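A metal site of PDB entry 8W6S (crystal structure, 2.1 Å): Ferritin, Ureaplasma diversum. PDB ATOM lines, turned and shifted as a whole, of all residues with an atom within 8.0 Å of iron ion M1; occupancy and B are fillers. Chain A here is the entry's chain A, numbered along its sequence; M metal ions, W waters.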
ATOM      1  N   ASN A  27      18.280  25.380  16.172  1.00  0.00           N
ATOM      2  CA  ASN A  27      18.943  24.699  15.056  1.00  0.00           C
ATOM      3  C   ASN A  27      18.918  25.543  13.794  1.00  0.00           C
ATOM      4  O   ASN A  27      19.876  25.525  13.013  1.00  0.00           O
ATOM      5  CB  ASN A  27      18.302  23.342  14.813  1.00  0.00           C
ATOM      6  CG  ASN A  27      18.904  22.273  15.690  1.00  0.00           C
ATOM      7  OD1 ASN A  27      20.001  21.801  15.438  1.00  0.00           O
ATOM      8  ND2 ASN A  27      18.196  21.910  16.749  1.00  0.00           N
ATOM      9  N   HIS A  56      28.938  21.690   6.069  1.00  0.00           N
ATOM     10  CA  HIS A  56      28.222  20.429   6.278  1.00  0.00           C
ATOM     11  C   HIS A  56      27.461  20.462   7.598  1.00  0.00           C
ATOM     12  O   HIS A  56      26.313  20.014   7.670  1.00  0.00           O
ATOM     13  CB  HIS A  56      29.193  19.254   6.249  1.00  0.00           C
ATOM     14  CG  HIS A  56      28.519  17.919   6.376  1.00  0.00           C
ATOM     15  ND1 HIS A  56      28.012  17.228   5.292  1.00  0.00           N
ATOM     16  CD2 HIS A  56      28.289  17.128   7.459  1.00  0.00           C
ATOM     17  CE1 HIS A  56      27.491  16.084   5.704  1.00  0.00           C
ATOM     18  NE2 HIS A  56      27.643  16.009   7.013  1.00  0.00           N
ATOM     19  N   LEU A  57      28.089  20.995   8.640  1.00  0.00           N
ATOM     20  CA  LEU A  57      27.394  21.137   9.913  1.00  0.00           C
ATOM     21  C   LEU A  57      26.210  22.103   9.795  1.00  0.00           C
ATOM     22  O   LEU A  57      25.147  21.855  10.369  1.00  0.00           O
ATOM     23  CB  LEU A  57      28.389  21.592  10.985  1.00  0.00           C
ATOM     24  CG  LEU A  57      27.953  21.521  12.458  1.00  0.00           C
ATOM     25  CD1 LEU A  57      27.506  20.122  12.825  1.00  0.00           C
ATOM     26  CD2 LEU A  57      29.111  21.970  13.343  1.00  0.00           C
ATOM     27  N   GLU A  59      24.265  22.642   7.140  1.00  0.00           N
ATOM     28  CA  GLU A  59      23.161  21.977   6.458  1.00  0.00           C
ATOM     29  C   GLU A  59      22.561  20.871   7.304  1.00  0.00           C
ATOM     30  O   GLU A  59      21.378  20.559   7.157  1.00  0.00           O
ATOM     31  CB  GLU A  59      23.652  21.425   5.119  1.00  0.00           C
ATOM     32  CG  GLU A  59      24.105  22.544   4.183  1.00  0.00           C
ATOM     33  CD  GLU A  59      24.926  22.056   2.995  1.00  0.00           C
ATOM     34  OE1 GLU A  59      25.344  22.920   2.193  1.00  0.00           O
ATOM     35  OE2 GLU A  59      25.151  20.839   2.861  1.00  0.00           O
ATOM     36  N   ASP A  60      23.365  20.263   8.171  1.00  0.00           N
ATOM     37  CA  ASP A  60      22.821  19.316   9.140  1.00  0.00           C
ATOM     38  C   ASP A  60      21.822  19.994  10.075  1.00  0.00           C
ATOM     39  O   ASP A  60      20.714  19.479  10.315  1.00  0.00           O
ATOM     40  CB  ASP A  60      23.974  18.706   9.927  1.00  0.00           C
ATOM     41  CG  ASP A  60      23.548  17.541  10.799  1.00  0.00           C
ATOM     42  OD1 ASP A  60      22.599  16.813  10.444  1.00  0.00           O
ATOM     43  OD2 ASP A  60      24.171  17.379  11.865  1.00  0.00           O
ATOM     44  N   LYS A  61      22.197  21.153  10.627  1.00  0.00           N
ATOM     45  CA  LYS A  61      21.310  21.831  11.580  1.00  0.00           C
ATOM     46  C   LYS A  61      20.035  22.310  10.902  1.00  0.00           C
ATOM     47  O   LYS A  61      18.941  22.175  11.465  1.00  0.00           O
ATOM     48  CB  LYS A  61      22.024  23.037  12.222  1.00  0.00           C
ATOM     49  CG  LYS A  61      23.303  22.730  13.023  1.00  0.00           C
ATOM     50  CD  LYS A  61      23.138  21.588  14.017  1.00  0.00           C
ATOM     51  CE  LYS A  61      24.377  21.477  14.900  1.00  0.00           C
ATOM     52  NZ  LYS A  61      24.297  20.397  15.939  1.00  0.00           N
ATOM     53  N   VAL A  64      18.052  17.828   8.820  1.00  0.00           N
ATOM     54  CA  VAL A  64      17.344  16.826   9.611  1.00  0.00           C
ATOM     55  C   VAL A  64      17.073  17.332  11.028  1.00  0.00           C
ATOM     56  O   VAL A  64      16.022  17.022  11.610  1.00  0.00           O
ATOM     57  CB  VAL A  64      18.105  15.485   9.614  1.00  0.00           C
ATOM     58  CG1 VAL A  64      18.176  14.924   8.199  1.00  0.00           C
ATOM     59  CG2 VAL A  64      19.506  15.643  10.222  1.00  0.00           C
ATOM     60  N   HIS A  65      17.995  18.098  11.603  1.00  0.00           N
ATOM     61  CA  HIS A  65      17.798  18.547  12.979  1.00  0.00           C
ATOM     62  C   HIS A  65      16.454  19.260  13.150  1.00  0.00           C
ATOM     63  O   HIS A  65      15.717  18.990  14.110  1.00  0.00           O
ATOM     64  CB  HIS A  65      18.941  19.460  13.423  1.00  0.00           C
ATOM     65  CG  HIS A  65      20.143  18.732  13.936  1.00  0.00           C
ATOM     66  ND1 HIS A  65      20.405  18.587  15.276  1.00  0.00           N
ATOM     67  CD2 HIS A  65      21.156  18.114  13.282  1.00  0.00           C
ATOM     68  CE1 HIS A  65      21.533  17.907  15.440  1.00  0.00           C
ATOM     69  NE2 HIS A  65      22.020  17.625  14.243  1.00  0.00           N
ATOM     70  N   GLU A 106      28.140  23.744  20.164  1.00  0.00           N
ATOM     71  CA  GLU A 106      27.723  22.340  20.198  1.00  0.00           C
ATOM     72  C   GLU A 106      27.621  21.831  21.627  1.00  0.00           C
ATOM     73  O   GLU A 106      26.734  21.032  21.950  1.00  0.00           O
ATOM     74  CB  GLU A 106      28.695  21.459  19.400  1.00  0.00           C
ATOM     75  CG  GLU A 106      28.673  21.717  17.895  1.00  0.00           C
ATOM     76  CD  GLU A 106      27.262  21.616  17.302  1.00  0.00           C
ATOM     77  OE1 GLU A 106      26.585  20.585  17.496  1.00  0.00           O
ATOM     78  OE2 GLU A 106      26.835  22.567  16.632  1.00  0.00           O
ATOM     79  N   VAL A 109      24.388  22.748  22.840  1.00  0.00           N
ATOM     80  CA  VAL A 109      23.342  21.878  22.306  1.00  0.00           C
ATOM     81  C   VAL A 109      23.114  20.694  23.247  1.00  0.00           C
ATOM     82  O   VAL A 109      21.979  20.388  23.632  1.00  0.00           O
ATOM     83  CB  VAL A 109      23.679  21.407  20.876  1.00  0.00           C
ATOM     84  CG1 VAL A 109      22.774  20.240  20.464  1.00  0.00           C
ATOM     85  CG2 VAL A 109      23.560  22.560  19.868  1.00  0.00           C
ATOM     86  N   TRP A 134      17.394  10.545  19.717  1.00  0.00           N
ATOM     87  CA  TRP A 134      18.160  10.888  18.516  1.00  0.00           C
ATOM     88  C   TRP A 134      19.019  12.110  18.761  1.00  0.00           C
ATOM     89  O   TRP A 134      20.190  12.158  18.372  1.00  0.00           O
ATOM     90  CB  TRP A 134      17.227  11.139  17.337  1.00  0.00           C
ATOM     91  CG  TRP A 134      17.957  11.336  16.014  1.00  0.00           C
ATOM     92  CD1 TRP A 134      18.233  10.371  15.077  1.00  0.00           C
ATOM     93  CD2 TRP A 134      18.497  12.560  15.489  1.00  0.00           C
ATOM     94  NE1 TRP A 134      18.916  10.912  14.016  1.00  0.00           N
ATOM     95  CE2 TRP A 134      19.080  12.262  14.235  1.00  0.00           C
ATOM     96  CE3 TRP A 134      18.531  13.886  15.955  1.00  0.00           C
ATOM     97  CZ2 TRP A 134      19.720  13.235  13.436  1.00  0.00           C
ATOM     98  CZ3 TRP A 134      19.163  14.864  15.158  1.00  0.00           C
ATOM     99  CH2 TRP A 134      19.739  14.531  13.915  1.00  0.00           C
ATOM    100  N   TYR A 135      18.445  13.114  19.429  1.00  0.00           N
ATOM    101  CA  TYR A 135      19.188  14.338  19.729  1.00  0.00           C
ATOM    102  C   TYR A 135      20.163  14.143  20.893  1.00  0.00           C
ATOM    103  O   TYR A 135      21.207  14.792  20.923  1.00  0.00           O
ATOM    104  CB  TYR A 135      18.193  15.454  20.035  1.00  0.00           C
ATOM    105  CG  TYR A 135      17.350  15.829  18.823  1.00  0.00           C
ATOM    106  CD1 TYR A 135      16.267  15.052  18.436  1.00  0.00           C
ATOM    107  CD2 TYR A 135      17.650  16.955  18.064  1.00  0.00           C
ATOM    108  CE1 TYR A 135      15.498  15.384  17.330  1.00  0.00           C
ATOM    109  CE2 TYR A 135      16.887  17.300  16.955  1.00  0.00           C
ATOM    110  CZ  TYR A 135      15.811  16.518  16.603  1.00  0.00           C
ATOM    111  OH  TYR A 135      15.042  16.851  15.497  1.00  0.00           O
ATOM    112  N   ARG A 137      21.872  11.328  21.332  1.00  0.00           N
ATOM    113  CA  ARG A 137      23.000  10.714  20.651  1.00  0.00           C
ATOM    114  C   ARG A 137      23.712  11.709  19.756  1.00  0.00           C
ATOM    115  O   ARG A 137      24.947  11.796  19.752  1.00  0.00           O
ATOM    116  CB  ARG A 137      22.526   9.505  19.836  1.00  0.00           C
ATOM    117  CG  ARG A 137      23.628   8.861  18.943  1.00  0.00           C
ATOM    118  CD  ARG A 137      23.038   8.186  17.683  1.00  0.00           C
ATOM    119  NE  ARG A 137      22.147   9.090  16.952  1.00  0.00           N
ATOM    120  CZ  ARG A 137      22.552  10.098  16.175  1.00  0.00           C
ATOM    121  NH1 ARG A 137      23.849  10.356  16.018  1.00  0.00           N
ATOM    122  NH2 ARG A 137      21.656  10.865  15.556  1.00  0.00           N
ATOM    123  N   ASP A 138      22.949  12.498  19.001  1.00  0.00           N
ATOM    124  CA  ASP A 138      23.580  13.390  18.032  1.00  0.00           C
ATOM    125  C   ASP A 138      24.313  14.534  18.708  1.00  0.00           C
ATOM    126  O   ASP A 138      25.274  15.068  18.134  1.00  0.00           O
ATOM    127  CB  ASP A 138      22.525  13.936  17.079  1.00  0.00           C
ATOM    128  CG  ASP A 138      23.121  14.334  15.741  1.00  0.00           C
ATOM    129  OD1 ASP A 138      23.431  13.428  14.938  1.00  0.00           O
ATOM    130  OD2 ASP A 138      23.284  15.540  15.511  1.00  0.00           O
ATOM    131  N   GLY A 139      23.872  14.932  19.908  1.00  0.00           N
ATOM    132  CA  GLY A 139      24.588  15.960  20.647  1.00  0.00           C
ATOM    133  C   GLY A 139      26.042  15.598  20.869  1.00  0.00           C
ATOM    134  O   GLY A 139      26.945  16.419  20.650  1.00  0.00           O
ATOM    135  N   LYS A 141      27.731  13.101  19.165  1.00  0.00           N
ATOM    136  CA  LYS A 141      28.364  12.825  17.873  1.00  0.00           C
ATOM    137  C   LYS A 141      28.866  14.106  17.209  1.00  0.00           C
ATOM    138  O   LYS A 141      30.029  14.175  16.784  1.00  0.00           O
ATOM    139  CB  LYS A 141      27.376  12.124  16.937  1.00  0.00           C
ATOM    140  CG  LYS A 141      28.014  11.743  15.584  1.00  0.00           C
ATOM    141  CD  LYS A 141      27.015  11.767  14.444  1.00  0.00           C
ATOM    142  CE  LYS A 141      26.634  13.183  14.074  1.00  0.00           C
ATOM    143  NZ  LYS A 141      26.308  13.372  12.618  1.00  0.00           N
ATOM    144  N   ASP A 142      28.007  15.115  17.089  1.00  0.00           N
ATOM    145  CA  ASP A 142      28.429  16.373  16.494  1.00  0.00           C
ATOM    146  C   ASP A 142      29.558  17.008  17.295  1.00  0.00           C
ATOM    147  O   ASP A 142      30.507  17.546  16.710  1.00  0.00           O
ATOM    148  CB  ASP A 142      27.256  17.351  16.386  1.00  0.00           C
ATOM    149  CG  ASP A 142      26.279  16.990  15.260  1.00  0.00           C
ATOM    150  OD1 ASP A 142      26.611  16.166  14.395  1.00  0.00           O
ATOM    151  OD2 ASP A 142      25.171  17.559  15.244  1.00  0.00           O
ATOM    152  N   LEU A 143      29.472  16.980  18.635  1.00  0.00           N
ATOM    153  CA  LEU A 143      30.559  17.524  19.440  1.00  0.00           C
ATOM    154  C   LEU A 143      31.876  16.812  19.166  1.00  0.00           C
ATOM    155  O   LEU A 143      32.942  17.439  19.146  1.00  0.00           O
ATOM    156  CB  LEU A 143      30.223  17.434  20.929  1.00  0.00           C
ATOM    157  CG  LEU A 143      31.279  18.116  21.802  1.00  0.00           C
ATOM    158  CD1 LEU A 143      31.044  19.621  21.879  1.00  0.00           C
ATOM    159  CD2 LEU A 143      31.380  17.504  23.191  1.00  0.00           C
ATOM    160  N   GLU A 145      32.779  15.237  16.352  1.00  0.00           N
ATOM    161  CA  GLU A 145      33.285  15.650  15.046  1.00  0.00           C
ATOM    162  C   GLU A 145      33.934  17.010  15.131  1.00  0.00           C
ATOM    163  O   GLU A 145      35.030  17.216  14.594  1.00  0.00           O
ATOM    164  CB  GLU A 145      32.155  15.630  14.013  1.00  0.00           C
ATOM    165  CG  GLU A 145      31.615  14.235  13.736  1.00  0.00           C
ATOM    166  CD  GLU A 145      30.581  14.193  12.617  1.00  0.00           C
ATOM    167  OE1 GLU A 145      30.098  15.267  12.185  1.00  0.00           O
ATOM    168  OE2 GLU A 145      30.242  13.064  12.178  1.00  0.00           O
HETATM  169 FE    FE M   1      23.796  16.530  13.812  1.00  0.00          FE
HETATM  170 FE    FE M   2      27.129  14.785   9.153  1.00  0.00          FE
HETATM  171  O   HOH W   1      23.441  14.845  12.529  1.00  0.00           O
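Iron ion M1 is bound by OD2 of Asp 138 (2.0 Å), NE2 of His 65 (2.1 Å), water W1 (2.1 Å), OD2 of Asp 60 (2.2 Å) and OD2 of Asp 142 (2.2 Å).
Within 4 Å of iron ion M1: Asp 60, His 65, Asp 138 and Asp 142.
Water W1 lies within hydrogen-bond range of OD1 of Asp 138 (2.8 Å), OD1 of Asp 60 (3.0 Å) and NZ of Lys 141 (3.2 Å).
O of His 65 lies within hydrogen-bond range of OH of Tyr 135 (2.6 Å). The guanidinium group (NH2) of Arg 137 is in salt-bridge range of the side-chain carboxylate (OD1) of Asp 138, at 3.2 Å. The side-chain amino group of Lys 141 lies within salt-bridge range of the side-chain carboxylate of Asp 142 (3.3 Å). The side-chain carboxylate (OD1) of Asp 138 lies within salt-bridge range of the side-chain amino group (NZ) of Lys 141. A ring nitrogen (ND1) of His 65 lies within hydrogen-bond range of the side-chain amide oxygen (OD1) of Asn 27 (3.2 Å). The side-chain amino group (NZ) of Lys 61 lies close to the side-chain carboxylate (OD2) of Asp 142 (3.0 Å).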
